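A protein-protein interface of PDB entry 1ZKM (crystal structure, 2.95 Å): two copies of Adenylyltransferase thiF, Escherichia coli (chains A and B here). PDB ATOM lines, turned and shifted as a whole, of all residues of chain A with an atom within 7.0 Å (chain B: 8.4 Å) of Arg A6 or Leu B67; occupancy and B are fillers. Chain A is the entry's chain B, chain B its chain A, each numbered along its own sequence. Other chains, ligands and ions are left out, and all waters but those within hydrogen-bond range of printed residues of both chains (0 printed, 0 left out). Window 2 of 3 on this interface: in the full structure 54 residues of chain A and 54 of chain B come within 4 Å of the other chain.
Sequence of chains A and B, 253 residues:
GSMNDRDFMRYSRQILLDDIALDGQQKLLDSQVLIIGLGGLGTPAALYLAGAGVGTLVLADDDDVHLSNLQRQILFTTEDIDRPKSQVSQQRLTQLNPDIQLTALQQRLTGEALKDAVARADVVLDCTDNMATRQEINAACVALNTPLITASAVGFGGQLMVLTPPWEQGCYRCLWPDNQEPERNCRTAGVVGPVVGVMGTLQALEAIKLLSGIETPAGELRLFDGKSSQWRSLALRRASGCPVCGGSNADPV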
ATOM      1  N   MET A   3      23.583  10.647 -30.620  1.00  0.00           N
ATOM      2  CA  MET A   3      24.035  10.484 -29.206  1.00  0.00           C
ATOM      3  C   MET A   3      24.998  11.599 -28.787  1.00  0.00           C
ATOM      4  O   MET A   3      26.204  11.511 -29.032  1.00  0.00           O
ATOM      5  CB  MET A   3      24.724   9.139 -29.033  1.00  0.00           C
ATOM      6  CG  MET A   3      24.985   8.806 -27.591  1.00  0.00           C
ATOM      7  SD  MET A   3      26.291   7.617 -27.414  1.00  0.00           S
ATOM      8  CE  MET A   3      27.703   8.678 -27.696  1.00  0.00           C
ATOM      9  N   ASN A   4      24.449  12.623 -28.130  1.00  0.00           N
ATOM     10  CA  ASN A   4      25.181  13.809 -27.667  1.00  0.00           C
ATOM     11  C   ASN A   4      26.199  13.651 -26.529  1.00  0.00           C
ATOM     12  O   ASN A   4      26.427  12.554 -26.020  1.00  0.00           O
ATOM     13  CB  ASN A   4      24.178  14.884 -27.258  1.00  0.00           C
ATOM     14  CG  ASN A   4      23.342  14.472 -26.062  1.00  0.00           C
ATOM     15  OD1 ASN A   4      23.879  14.053 -25.037  1.00  0.00           O
ATOM     16  ND2 ASN A   4      22.024  14.595 -26.183  1.00  0.00           N
ATOM     17  N   ASP A   5      26.796  14.778 -26.136  1.00  0.00           N
ATOM     18  CA  ASP A   5      27.792  14.833 -25.065  1.00  0.00           C
ATOM     19  C   ASP A   5      27.267  14.242 -23.763  1.00  0.00           C
ATOM     20  O   ASP A   5      27.947  13.443 -23.110  1.00  0.00           O
ATOM     21  CB  ASP A   5      28.220  16.282 -24.811  1.00  0.00           C
ATOM     22  CG  ASP A   5      29.387  16.715 -25.679  1.00  0.00           C
ATOM     23  OD1 ASP A   5      29.881  15.894 -26.488  1.00  0.00           O
ATOM     24  OD2 ASP A   5      29.818  17.884 -25.540  1.00  0.00           O
ATOM     25  N   ARG A   6      26.058  14.657 -23.386  1.00  0.00           N
ATOM     26  CA  ARG A   6      25.406  14.183 -22.168  1.00  0.00           C
ATOM     27  C   ARG A   6      25.278  12.657 -22.201  1.00  0.00           C
ATOM     28  O   ARG A   6      25.772  11.955 -21.317  1.00  0.00           O
ATOM     29  CB  ARG A   6      24.023  14.821 -22.046  1.00  0.00           C
ATOM     30  CG  ARG A   6      23.219  14.311 -20.885  1.00  0.00           C
ATOM     31  CD  ARG A   6      21.824  14.874 -20.902  1.00  0.00           C
ATOM     32  NE  ARG A   6      21.040  14.355 -19.787  1.00  0.00           N
ATOM     33  CZ  ARG A   6      19.768  14.665 -19.554  1.00  0.00           C
ATOM     34  NH1 ARG A   6      19.126  15.501 -20.365  1.00  0.00           N
ATOM     35  NH2 ARG A   6      19.140  14.141 -18.510  1.00  0.00           N
ATOM     36  N   ASP A   7      24.616  12.150 -23.235  1.00  0.00           N
ATOM     37  CA  ASP A   7      24.431  10.717 -23.382  1.00  0.00           C
ATOM     38  C   ASP A   7      25.753   9.966 -23.351  1.00  0.00           C
ATOM     39  O   ASP A   7      25.893   8.997 -22.603  1.00  0.00           O
ATOM     40  CB  ASP A   7      23.667  10.422 -24.666  1.00  0.00           C
ATOM     41  CG  ASP A   7      22.247  10.940 -24.611  1.00  0.00           C
ATOM     42  OD1 ASP A   7      21.555  10.634 -23.618  1.00  0.00           O
ATOM     43  OD2 ASP A   7      21.819  11.649 -25.544  1.00  0.00           O
ATOM     44  N   PHE A   8      26.726  10.400 -24.144  1.00  0.00           N
ATOM     45  CA  PHE A   8      28.013   9.721 -24.116  1.00  0.00           C
ATOM     46  C   PHE A   8      28.523   9.648 -22.684  1.00  0.00           C
ATOM     47  O   PHE A   8      29.095   8.641 -22.269  1.00  0.00           O
ATOM     48  CB  PHE A   8      29.082  10.443 -24.942  1.00  0.00           C
ATOM     49  CG  PHE A   8      30.488  10.007 -24.595  1.00  0.00           C
ATOM     50  CD1 PHE A   8      31.017   8.832 -25.115  1.00  0.00           C
ATOM     51  CD2 PHE A   8      31.243  10.720 -23.660  1.00  0.00           C
ATOM     52  CE1 PHE A   8      32.279   8.362 -24.702  1.00  0.00           C
ATOM     53  CE2 PHE A   8      32.502  10.261 -23.241  1.00  0.00           C
ATOM     54  CZ  PHE A   8      33.021   9.078 -23.761  1.00  0.00           C
ATOM     55  N   MET A   9      28.333  10.724 -21.931  1.00  0.00           N
ATOM     56  CA  MET A   9      28.813  10.740 -20.561  1.00  0.00           C
ATOM     57  C   MET A   9      28.134   9.754 -19.615  1.00  0.00           C
ATOM     58  O   MET A   9      28.820   9.024 -18.899  1.00  0.00           O
ATOM     59  CB  MET A   9      28.727  12.149 -19.983  1.00  0.00           C
ATOM     60  CG  MET A   9      30.083  12.811 -19.851  1.00  0.00           C
ATOM     61  SD  MET A   9      31.219  11.768 -18.929  1.00  0.00           S
ATOM     62  CE  MET A   9      32.761  12.166 -19.706  1.00  0.00           C
ATOM     63  N   ARG A  10      26.803   9.707 -19.602  1.00  0.00           N
ATOM     64  CA  ARG A  10      26.163   8.785 -18.683  1.00  0.00           C
ATOM     65  C   ARG A  10      26.449   7.333 -19.023  1.00  0.00           C
ATOM     66  O   ARG A  10      26.864   6.567 -18.149  1.00  0.00           O
ATOM     67  CB  ARG A  10      24.655   9.035 -18.580  1.00  0.00           C
ATOM     68  CG  ARG A  10      23.787   8.576 -19.720  1.00  0.00           C
ATOM     69  CD  ARG A  10      22.330   8.586 -19.249  1.00  0.00           C
ATOM     70  NE  ARG A  10      22.018   9.812 -18.504  1.00  0.00           N
ATOM     71  CZ  ARG A  10      21.243   9.867 -17.420  1.00  0.00           C
ATOM     72  NH1 ARG A  10      20.688   8.763 -16.935  1.00  0.00           N
ATOM     73  NH2 ARG A  10      21.033  11.029 -16.814  1.00  0.00           N
ATOM     74  N   TYR A  11      26.277   6.958 -20.288  1.00  0.00           N
ATOM     75  CA  TYR A  11      26.520   5.575 -20.695  1.00  0.00           C
ATOM     76  C   TYR A  11      27.994   5.226 -20.908  1.00  0.00           C
ATOM     77  O   TYR A  11      28.329   4.095 -21.275  1.00  0.00           O
ATOM     78  CB  TYR A  11      25.726   5.265 -21.956  1.00  0.00           C
ATOM     79  CG  TYR A  11      24.262   5.585 -21.803  1.00  0.00           C
ATOM     80  CD1 TYR A  11      23.615   6.404 -22.715  1.00  0.00           C
ATOM     81  CD2 TYR A  11      23.532   5.095 -20.729  1.00  0.00           C
ATOM     82  CE1 TYR A  11      22.279   6.733 -22.563  1.00  0.00           C
ATOM     83  CE2 TYR A  11      22.198   5.414 -20.564  1.00  0.00           C
ATOM     84  CZ  TYR A  11      21.574   6.237 -21.483  1.00  0.00           C
ATOM     85  OH  TYR A  11      20.250   6.584 -21.326  1.00  0.00           O
ATOM     86  N   SER A  12      28.873   6.179 -20.625  1.00  0.00           N
ATOM     87  CA  SER A  12      30.295   5.974 -20.843  1.00  0.00           C
ATOM     88  C   SER A  12      30.930   4.738 -20.236  1.00  0.00           C
ATOM     89  O   SER A  12      31.856   4.185 -20.828  1.00  0.00           O
ATOM     90  CB  SER A  12      31.084   7.208 -20.409  1.00  0.00           C
ATOM     91  OG  SER A  12      31.000   7.408 -19.017  1.00  0.00           O
ATOM     92  N   THR A  94      12.509   8.441 -13.339  1.00  0.00           N
ATOM     93  CA  THR A  94      12.714   9.569 -14.229  1.00  0.00           C
ATOM     94  C   THR A  94      13.790  10.500 -13.680  1.00  0.00           C
ATOM     95  O   THR A  94      14.585  11.044 -14.431  1.00  0.00           O
ATOM     96  CB  THR A  94      11.418  10.377 -14.448  1.00  0.00           C
ATOM     97  OG1 THR A  94      10.503   9.608 -15.240  1.00  0.00           O
ATOM     98  CG2 THR A  94      11.720  11.675 -15.177  1.00  0.00           C
ATOM     99  N   LEU A  96      16.315   9.718 -12.321  1.00  0.00           N
ATOM    100  CA  LEU A  96      17.588   9.038 -12.575  1.00  0.00           C
ATOM    101  C   LEU A  96      17.976   9.089 -14.047  1.00  0.00           C
ATOM    102  O   LEU A  96      19.151   9.220 -14.396  1.00  0.00           O
ATOM    103  CB  LEU A  96      17.487   7.574 -12.132  1.00  0.00           C
ATOM    104  CG  LEU A  96      18.663   6.661 -12.486  1.00  0.00           C
ATOM    105  CD1 LEU A  96      19.918   7.146 -11.775  1.00  0.00           C
ATOM    106  CD2 LEU A  96      18.344   5.236 -12.093  1.00  0.00           C
ATOM    107  N   ASN A  97      16.972   8.967 -14.903  1.00  0.00           N
ATOM    108  CA  ASN A  97      17.187   8.988 -16.331  1.00  0.00           C
ATOM    109  C   ASN A  97      15.950   9.543 -17.033  1.00  0.00           C
ATOM    110  O   ASN A  97      15.035   8.799 -17.408  1.00  0.00           O
ATOM    111  CB  ASN A  97      17.471   7.585 -16.828  1.00  0.00           C
ATOM    112  CG  ASN A  97      18.116   7.584 -18.174  1.00  0.00           C
ATOM    113  OD1 ASN A  97      17.690   8.301 -19.070  1.00  0.00           O
ATOM    114  ND2 ASN A  97      19.153   6.775 -18.333  1.00  0.00           N
ATOM    115  N   PRO A  98      15.908  10.870 -17.218  1.00  0.00           N
ATOM    116  CA  PRO A  98      14.794  11.565 -17.873  1.00  0.00           C
ATOM    117  C   PRO A  98      14.819  11.303 -19.368  1.00  0.00           C
ATOM    118  O   PRO A  98      13.829  11.501 -20.067  1.00  0.00           O
ATOM    119  CB  PRO A  98      15.081  13.032 -17.583  1.00  0.00           C
ATOM    120  CG  PRO A  98      16.050  13.002 -16.412  1.00  0.00           C
ATOM    121  CD  PRO A  98      16.906  11.831 -16.721  1.00  0.00           C
ATOM    122  N   ASP A  99      15.978  10.861 -19.843  1.00  0.00           N
ATOM    123  CA  ASP A  99      16.183  10.598 -21.254  1.00  0.00           C
ATOM    124  C   ASP A  99      15.710   9.239 -21.760  1.00  0.00           C
ATOM    125  O   ASP A  99      16.158   8.791 -22.818  1.00  0.00           O
ATOM    126  CB  ASP A  99      17.661  10.770 -21.597  1.00  0.00           C
ATOM    127  CG  ASP A  99      18.236  12.065 -21.058  1.00  0.00           C
ATOM    128  OD1 ASP A  99      17.510  13.088 -21.069  1.00  0.00           O
ATOM    129  OD2 ASP A  99      19.421  12.055 -20.639  1.00  0.00           O
ATOM    130  N   ASP B  64      31.900  13.755  -5.440  1.00  0.00           N
ATOM    131  CA  ASP B  64      30.578  14.295  -5.767  1.00  0.00           C
ATOM    132  C   ASP B  64      29.789  13.377  -6.718  1.00  0.00           C
ATOM    133  O   ASP B  64      30.304  12.386  -7.204  1.00  0.00           O
ATOM    134  CB  ASP B  64      30.707  15.689  -6.398  1.00  0.00           C
ATOM    135  CG  ASP B  64      31.173  16.748  -5.406  1.00  0.00           C
ATOM    136  OD1 ASP B  64      30.551  16.888  -4.330  1.00  0.00           O
ATOM    137  OD2 ASP B  64      32.158  17.453  -5.707  1.00  0.00           O
ATOM    138  N   VAL B  65      28.532  13.706  -6.971  1.00  0.00           N
ATOM    139  CA  VAL B  65      27.703  12.898  -7.855  1.00  0.00           C
ATOM    140  C   VAL B  65      27.913  13.379  -9.283  1.00  0.00           C
ATOM    141  O   VAL B  65      27.651  14.542  -9.596  1.00  0.00           O
ATOM    142  CB  VAL B  65      26.202  13.042  -7.494  1.00  0.00           C
ATOM    143  CG1 VAL B  65      25.341  12.128  -8.361  1.00  0.00           C
ATOM    144  CG2 VAL B  65      26.007  12.736  -6.024  1.00  0.00           C
ATOM    145  N   HIS B  66      28.385  12.485 -10.149  1.00  0.00           N
ATOM    146  CA  HIS B  66      28.628  12.823 -11.547  1.00  0.00           C
ATOM    147  C   HIS B  66      27.741  11.997 -12.464  1.00  0.00           C
ATOM    148  O   HIS B  66      27.430  10.845 -12.167  1.00  0.00           O
ATOM    149  CB  HIS B  66      30.090  12.581 -11.897  1.00  0.00           C
ATOM    150  CG  HIS B  66      31.045  13.333 -11.026  1.00  0.00           C
ATOM    151  ND1 HIS B  66      30.990  14.703 -10.872  1.00  0.00           N
ATOM    152  CD2 HIS B  66      32.079  12.907 -10.261  1.00  0.00           C
ATOM    153  CE1 HIS B  66      31.950  15.088 -10.049  1.00  0.00           C
ATOM    154  NE2 HIS B  66      32.625  14.017  -9.665  1.00  0.00           N
ATOM    155  N   LEU B  67      27.341  12.591 -13.581  1.00  0.00           N
ATOM    156  CA  LEU B  67      26.480  11.912 -14.538  1.00  0.00           C
ATOM    157  C   LEU B  67      27.008  10.517 -14.864  1.00  0.00           C
ATOM    158  O   LEU B  67      26.235   9.577 -15.047  1.00  0.00           O
ATOM    159  CB  LEU B  67      26.364  12.755 -15.802  1.00  0.00           C
ATOM    160  CG  LEU B  67      25.439  12.243 -16.905  1.00  0.00           C
ATOM    161  CD1 LEU B  67      23.978  12.278 -16.463  1.00  0.00           C
ATOM    162  CD2 LEU B  67      25.633  13.110 -18.139  1.00  0.00           C
ATOM    163  N   SER B  68      28.328  10.388 -14.908  1.00  0.00           N
ATOM    164  CA  SER B  68      28.986   9.112 -15.201  1.00  0.00           C
ATOM    165  C   SER B  68      28.586   8.014 -14.217  1.00  0.00           C
ATOM    166  O   SER B  68      28.641   6.823 -14.538  1.00  0.00           O
ATOM    167  CB  SER B  68      30.503   9.289 -15.140  1.00  0.00           C
ATOM    168  OG  SER B  68      30.849  10.670 -15.051  1.00  0.00           O
ATOM    169  N   ASN B  69      28.177   8.429 -13.019  1.00  0.00           N
ATOM    170  CA  ASN B  69      27.797   7.519 -11.937  1.00  0.00           C
ATOM    171  C   ASN B  69      26.423   6.882 -12.031  1.00  0.00           C
ATOM    172  O   ASN B  69      26.253   5.687 -11.794  1.00  0.00           O
ATOM    173  CB  ASN B  69      27.872   8.254 -10.599  1.00  0.00           C
ATOM    174  CG  ASN B  69      29.211   8.906 -10.363  1.00  0.00           C
ATOM    175  OD1 ASN B  69      30.258   8.328 -10.660  1.00  0.00           O
ATOM    176  ND2 ASN B  69      29.190  10.112  -9.809  1.00  0.00           N
ATOM    177  N   LEU B  70      25.440   7.698 -12.366  1.00  0.00           N
ATOM    178  CA  LEU B  70      24.067   7.245 -12.438  1.00  0.00           C
ATOM    179  C   LEU B  70      23.787   5.896 -13.089  1.00  0.00           C
ATOM    180  O   LEU B  70      22.714   5.346 -12.893  1.00  0.00           O
ATOM    181  CB  LEU B  70      23.216   8.317 -13.109  1.00  0.00           C
ATOM    182  CG  LEU B  70      23.539   9.742 -12.660  1.00  0.00           C
ATOM    183  CD1 LEU B  70      22.394  10.643 -13.107  1.00  0.00           C
ATOM    184  CD2 LEU B  70      23.724   9.822 -11.147  1.00  0.00           C
ATOM    185  N   GLN B  71      24.715   5.341 -13.851  1.00  0.00           N
ATOM    186  CA  GLN B  71      24.414   4.063 -14.485  1.00  0.00           C
ATOM    187  C   GLN B  71      24.565   2.845 -13.573  1.00  0.00           C
ATOM    188  O   GLN B  71      24.095   1.755 -13.911  1.00  0.00           O
ATOM    189  CB  GLN B  71      25.274   3.874 -15.731  1.00  0.00           C
ATOM    190  CG  GLN B  71      26.668   3.316 -15.468  1.00  0.00           C
ATOM    191  CD  GLN B  71      26.786   1.898 -15.971  1.00  0.00           C
ATOM    192  OE1 GLN B  71      25.909   1.424 -16.693  1.00  0.00           O
ATOM    193  NE2 GLN B  71      27.869   1.216 -15.617  1.00  0.00           N
ATOM    194  N   ARG B  72      25.208   3.018 -12.422  1.00  0.00           N
ATOM    195  CA  ARG B  72      25.394   1.898 -11.511  1.00  0.00           C
ATOM    196  C   ARG B  72      25.233   2.274 -10.037  1.00  0.00           C
ATOM    197  O   ARG B  72      24.986   1.411  -9.178  1.00  0.00           O
ATOM    198  CB  ARG B  72      26.768   1.245 -11.733  1.00  0.00           C
ATOM    199  CG  ARG B  72      27.968   2.176 -11.621  1.00  0.00           C
ATOM    200  CD  ARG B  72      28.508   2.489 -13.008  1.00  0.00           C
ATOM    201  NE  ARG B  72      29.357   3.675 -13.058  1.00  0.00           N
ATOM    202  CZ  ARG B  72      30.479   3.821 -12.360  1.00  0.00           C
ATOM    203  NH1 ARG B  72      30.897   2.847 -11.550  1.00  0.00           N
ATOM    204  NH2 ARG B  72      31.177   4.947 -12.470  1.00  0.00           N
ATOM    205  N   GLN B  73      25.394   3.559  -9.748  1.00  0.00           N
ATOM    206  CA  GLN B  73      25.258   4.078  -8.392  1.00  0.00           C
ATOM    207  C   GLN B  73      23.792   4.483  -8.291  1.00  0.00           C
ATOM    208  O   GLN B  73      23.435   5.658  -8.394  1.00  0.00           O
ATOM    209  CB  GLN B  73      26.206   5.270  -8.207  1.00  0.00           C
ATOM    210  CG  GLN B  73      27.677   4.875  -8.403  1.00  0.00           C
ATOM    211  CD  GLN B  73      28.669   6.035  -8.299  1.00  0.00           C
ATOM    212  OE1 GLN B  73      28.357   7.098  -7.754  1.00  0.00           O
ATOM    213  NE2 GLN B  73      29.884   5.823  -8.807  1.00  0.00           N
ATOM    214  N   THR B  77      20.408  10.384  -8.058  1.00  0.00           N
ATOM    215  CA  THR B  77      19.462  10.825  -9.073  1.00  0.00           C
ATOM    216  C   THR B  77      20.190  11.924  -9.860  1.00  0.00           C
ATOM    217  O   THR B  77      21.155  12.506  -9.344  1.00  0.00           O
ATOM    218  CB  THR B  77      18.184  11.381  -8.381  1.00  0.00           C
ATOM    219  OG1 THR B  77      17.063  11.232  -9.245  1.00  0.00           O
ATOM    220  CG2 THR B  77      18.337  12.853  -8.045  1.00  0.00           C
ATOM    221  N   THR B  78      19.753  12.214 -11.088  1.00  0.00           N
ATOM    222  CA  THR B  78      20.439  13.242 -11.885  1.00  0.00           C
ATOM    223  C   THR B  78      20.471  14.585 -11.153  1.00  0.00           C
ATOM    224  O   THR B  78      21.468  15.306 -11.217  1.00  0.00           O
ATOM    225  CB  THR B  78      19.786  13.463 -13.285  1.00  0.00           C
ATOM    226  OG1 THR B  78      18.608  14.262 -13.146  1.00  0.00           O
ATOM    227  CG2 THR B  78      19.407  12.135 -13.922  1.00  0.00           C
ATOM    228  N   GLU B  79      19.379  14.903 -10.455  1.00  0.00           N
ATOM    229  CA  GLU B  79      19.254  16.150  -9.698  1.00  0.00           C
ATOM    230  C   GLU B  79      20.325  16.296  -8.607  1.00  0.00           C
ATOM    231  O   GLU B  79      20.560  17.393  -8.108  1.00  0.00           O
ATOM    232  CB  GLU B  79      17.876  16.217  -9.049  1.00  0.00           C
ATOM    233  CG  GLU B  79      16.764  15.700  -9.931  1.00  0.00           C
ATOM    234  CD  GLU B  79      15.446  15.587  -9.190  1.00  0.00           C
ATOM    235  OE1 GLU B  79      15.432  14.986  -8.091  1.00  0.00           O
ATOM    236  OE2 GLU B  79      14.423  16.087  -9.708  1.00  0.00           O
ATOM    237  N   ASP B  80      20.976  15.194  -8.246  1.00  0.00           N
ATOM    238  CA  ASP B  80      22.001  15.211  -7.209  1.00  0.00           C
ATOM    239  C   ASP B  80      23.392  15.503  -7.749  1.00  0.00           C
ATOM    240  O   ASP B  80      24.372  15.505  -7.002  1.00  0.00           O
ATOM    241  CB  ASP B  80      22.047  13.859  -6.481  1.00  0.00           C
ATOM    242  CG  ASP B  80      20.729  13.491  -5.833  1.00  0.00           C
ATOM    243  OD1 ASP B  80      20.156  14.318  -5.091  1.00  0.00           O
ATOM    244  OD2 ASP B  80      20.268  12.359  -6.058  1.00  0.00           O
ATOM    245  N   ILE B  81      23.493  15.742  -9.045  1.00  0.00           N
ATOM    246  CA  ILE B  81      24.799  15.977  -9.630  1.00  0.00           C
ATOM    247  C   ILE B  81      25.584  17.112  -8.986  1.00  0.00           C
ATOM    248  O   ILE B  81      25.036  18.156  -8.654  1.00  0.00           O
ATOM    249  CB  ILE B  81      24.676  16.188 -11.153  1.00  0.00           C
ATOM    250  CG1 ILE B  81      24.254  14.863 -11.804  1.00  0.00           C
ATOM    251  CG2 ILE B  81      25.997  16.650 -11.726  1.00  0.00           C
ATOM    252  CD1 ILE B  81      24.011  14.912 -13.287  1.00  0.00           C
ATOM    253  N   ASP B  82      26.875  16.878  -8.795  1.00  0.00           N
ATOM    254  CA  ASP B  82      27.787  17.849  -8.194  1.00  0.00           C
ATOM    255  C   ASP B  82      27.622  18.062  -6.703  1.00  0.00           C
ATOM    256  O   ASP B  82      28.307  18.892  -6.103  1.00  0.00           O
ATOM    257  CB  ASP B  82      27.704  19.184  -8.923  1.00  0.00           C
ATOM    258  CG  ASP B  82      28.635  19.241 -10.111  1.00  0.00           C
ATOM    259  OD1 ASP B  82      29.852  18.998  -9.918  1.00  0.00           O
ATOM    260  OD2 ASP B  82      28.154  19.524 -11.230  1.00  0.00           O
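Of the 16 printed residues of chain B, 6 touch a printed residue of chain A. Hydrophobic or aromatic side chains of chain B that line the printed part of chain A: Leu B67 and Leu B70. Of the 15 printed residues of chain A, 5 touch a printed residue of chain B. Printed residues of chain A that touch a printed residue of chain B: Arg A6, Met A9, Arg A10, Leu A96 and Pro A98. Among the printed residues, 11 pairs touch across the chains. Among the printed residues, no Asp or Glu carboxylate lies within 4 Å of a Lys or Arg side-chain nitrogen of the other chain.
No position is printed for both chains.
The guanidinium group of Arg A10 sits close to the side-chain amide nitrogen of Asn A97, at 2.9 Å. The guanidinium group (NH1) of Arg A10 is in hydrogen-bond range of the backbone carbonyl oxygen (O) of Leu A96. The side-chain carboxylate (OD2) of Asp A99 is in salt-bridge range of the guanidinium group (NE) of Arg A6, 2.9 Å away. N of Arg A6 lies within hydrogen-bond range of OD1 of Asn A4. The backbone carbonyl oxygen (O) of Met A9 sits at hydrogen-bond distance from the side-chain hydroxyl (OG) of Ser A12, at 2.7 Å. The side-chain carboxylate of Asp B80 lies within hydrogen-bond range of the backbone NH of Thr B77 (2.8 Å).
Among the printed residues, merely in contact across the chains: Arg A6 with Leu B67, Met A9 with Leu B67, Met A9 with Ser B68, Arg A10 with Leu B67, Arg A10 with Leu B70, Arg A10 with Gln B71, Arg A10 with Thr B78, Leu A96 with Leu B70, Leu A96 with Thr B77, Leu A96 with Thr B78 and Pro A98 with Thr B78.
Arg A6 touches one residue of chain B. Leu B67 touches just these residues of chain A: Arg A6, Met A9 and Arg A10. Of the printed residues of chain A, Gln B71 touches Arg A10. Printed residues of chain A within 4 Å of Ser B68: Met A9 (3.7 Å). Of the printed residues of chain B, Met A9 touches Leu B67 and Ser B68. Printed residues of chain B within 4 Å of Leu A96: Leu B70, Thr B77 and Thr B78. Of the printed residues of chain A, Thr B78 touches Arg A10, Leu A96 and Pro A98. The nearest printed residue of chain B that does not touch Leu A96 is Gln B73 (5.1 Å).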
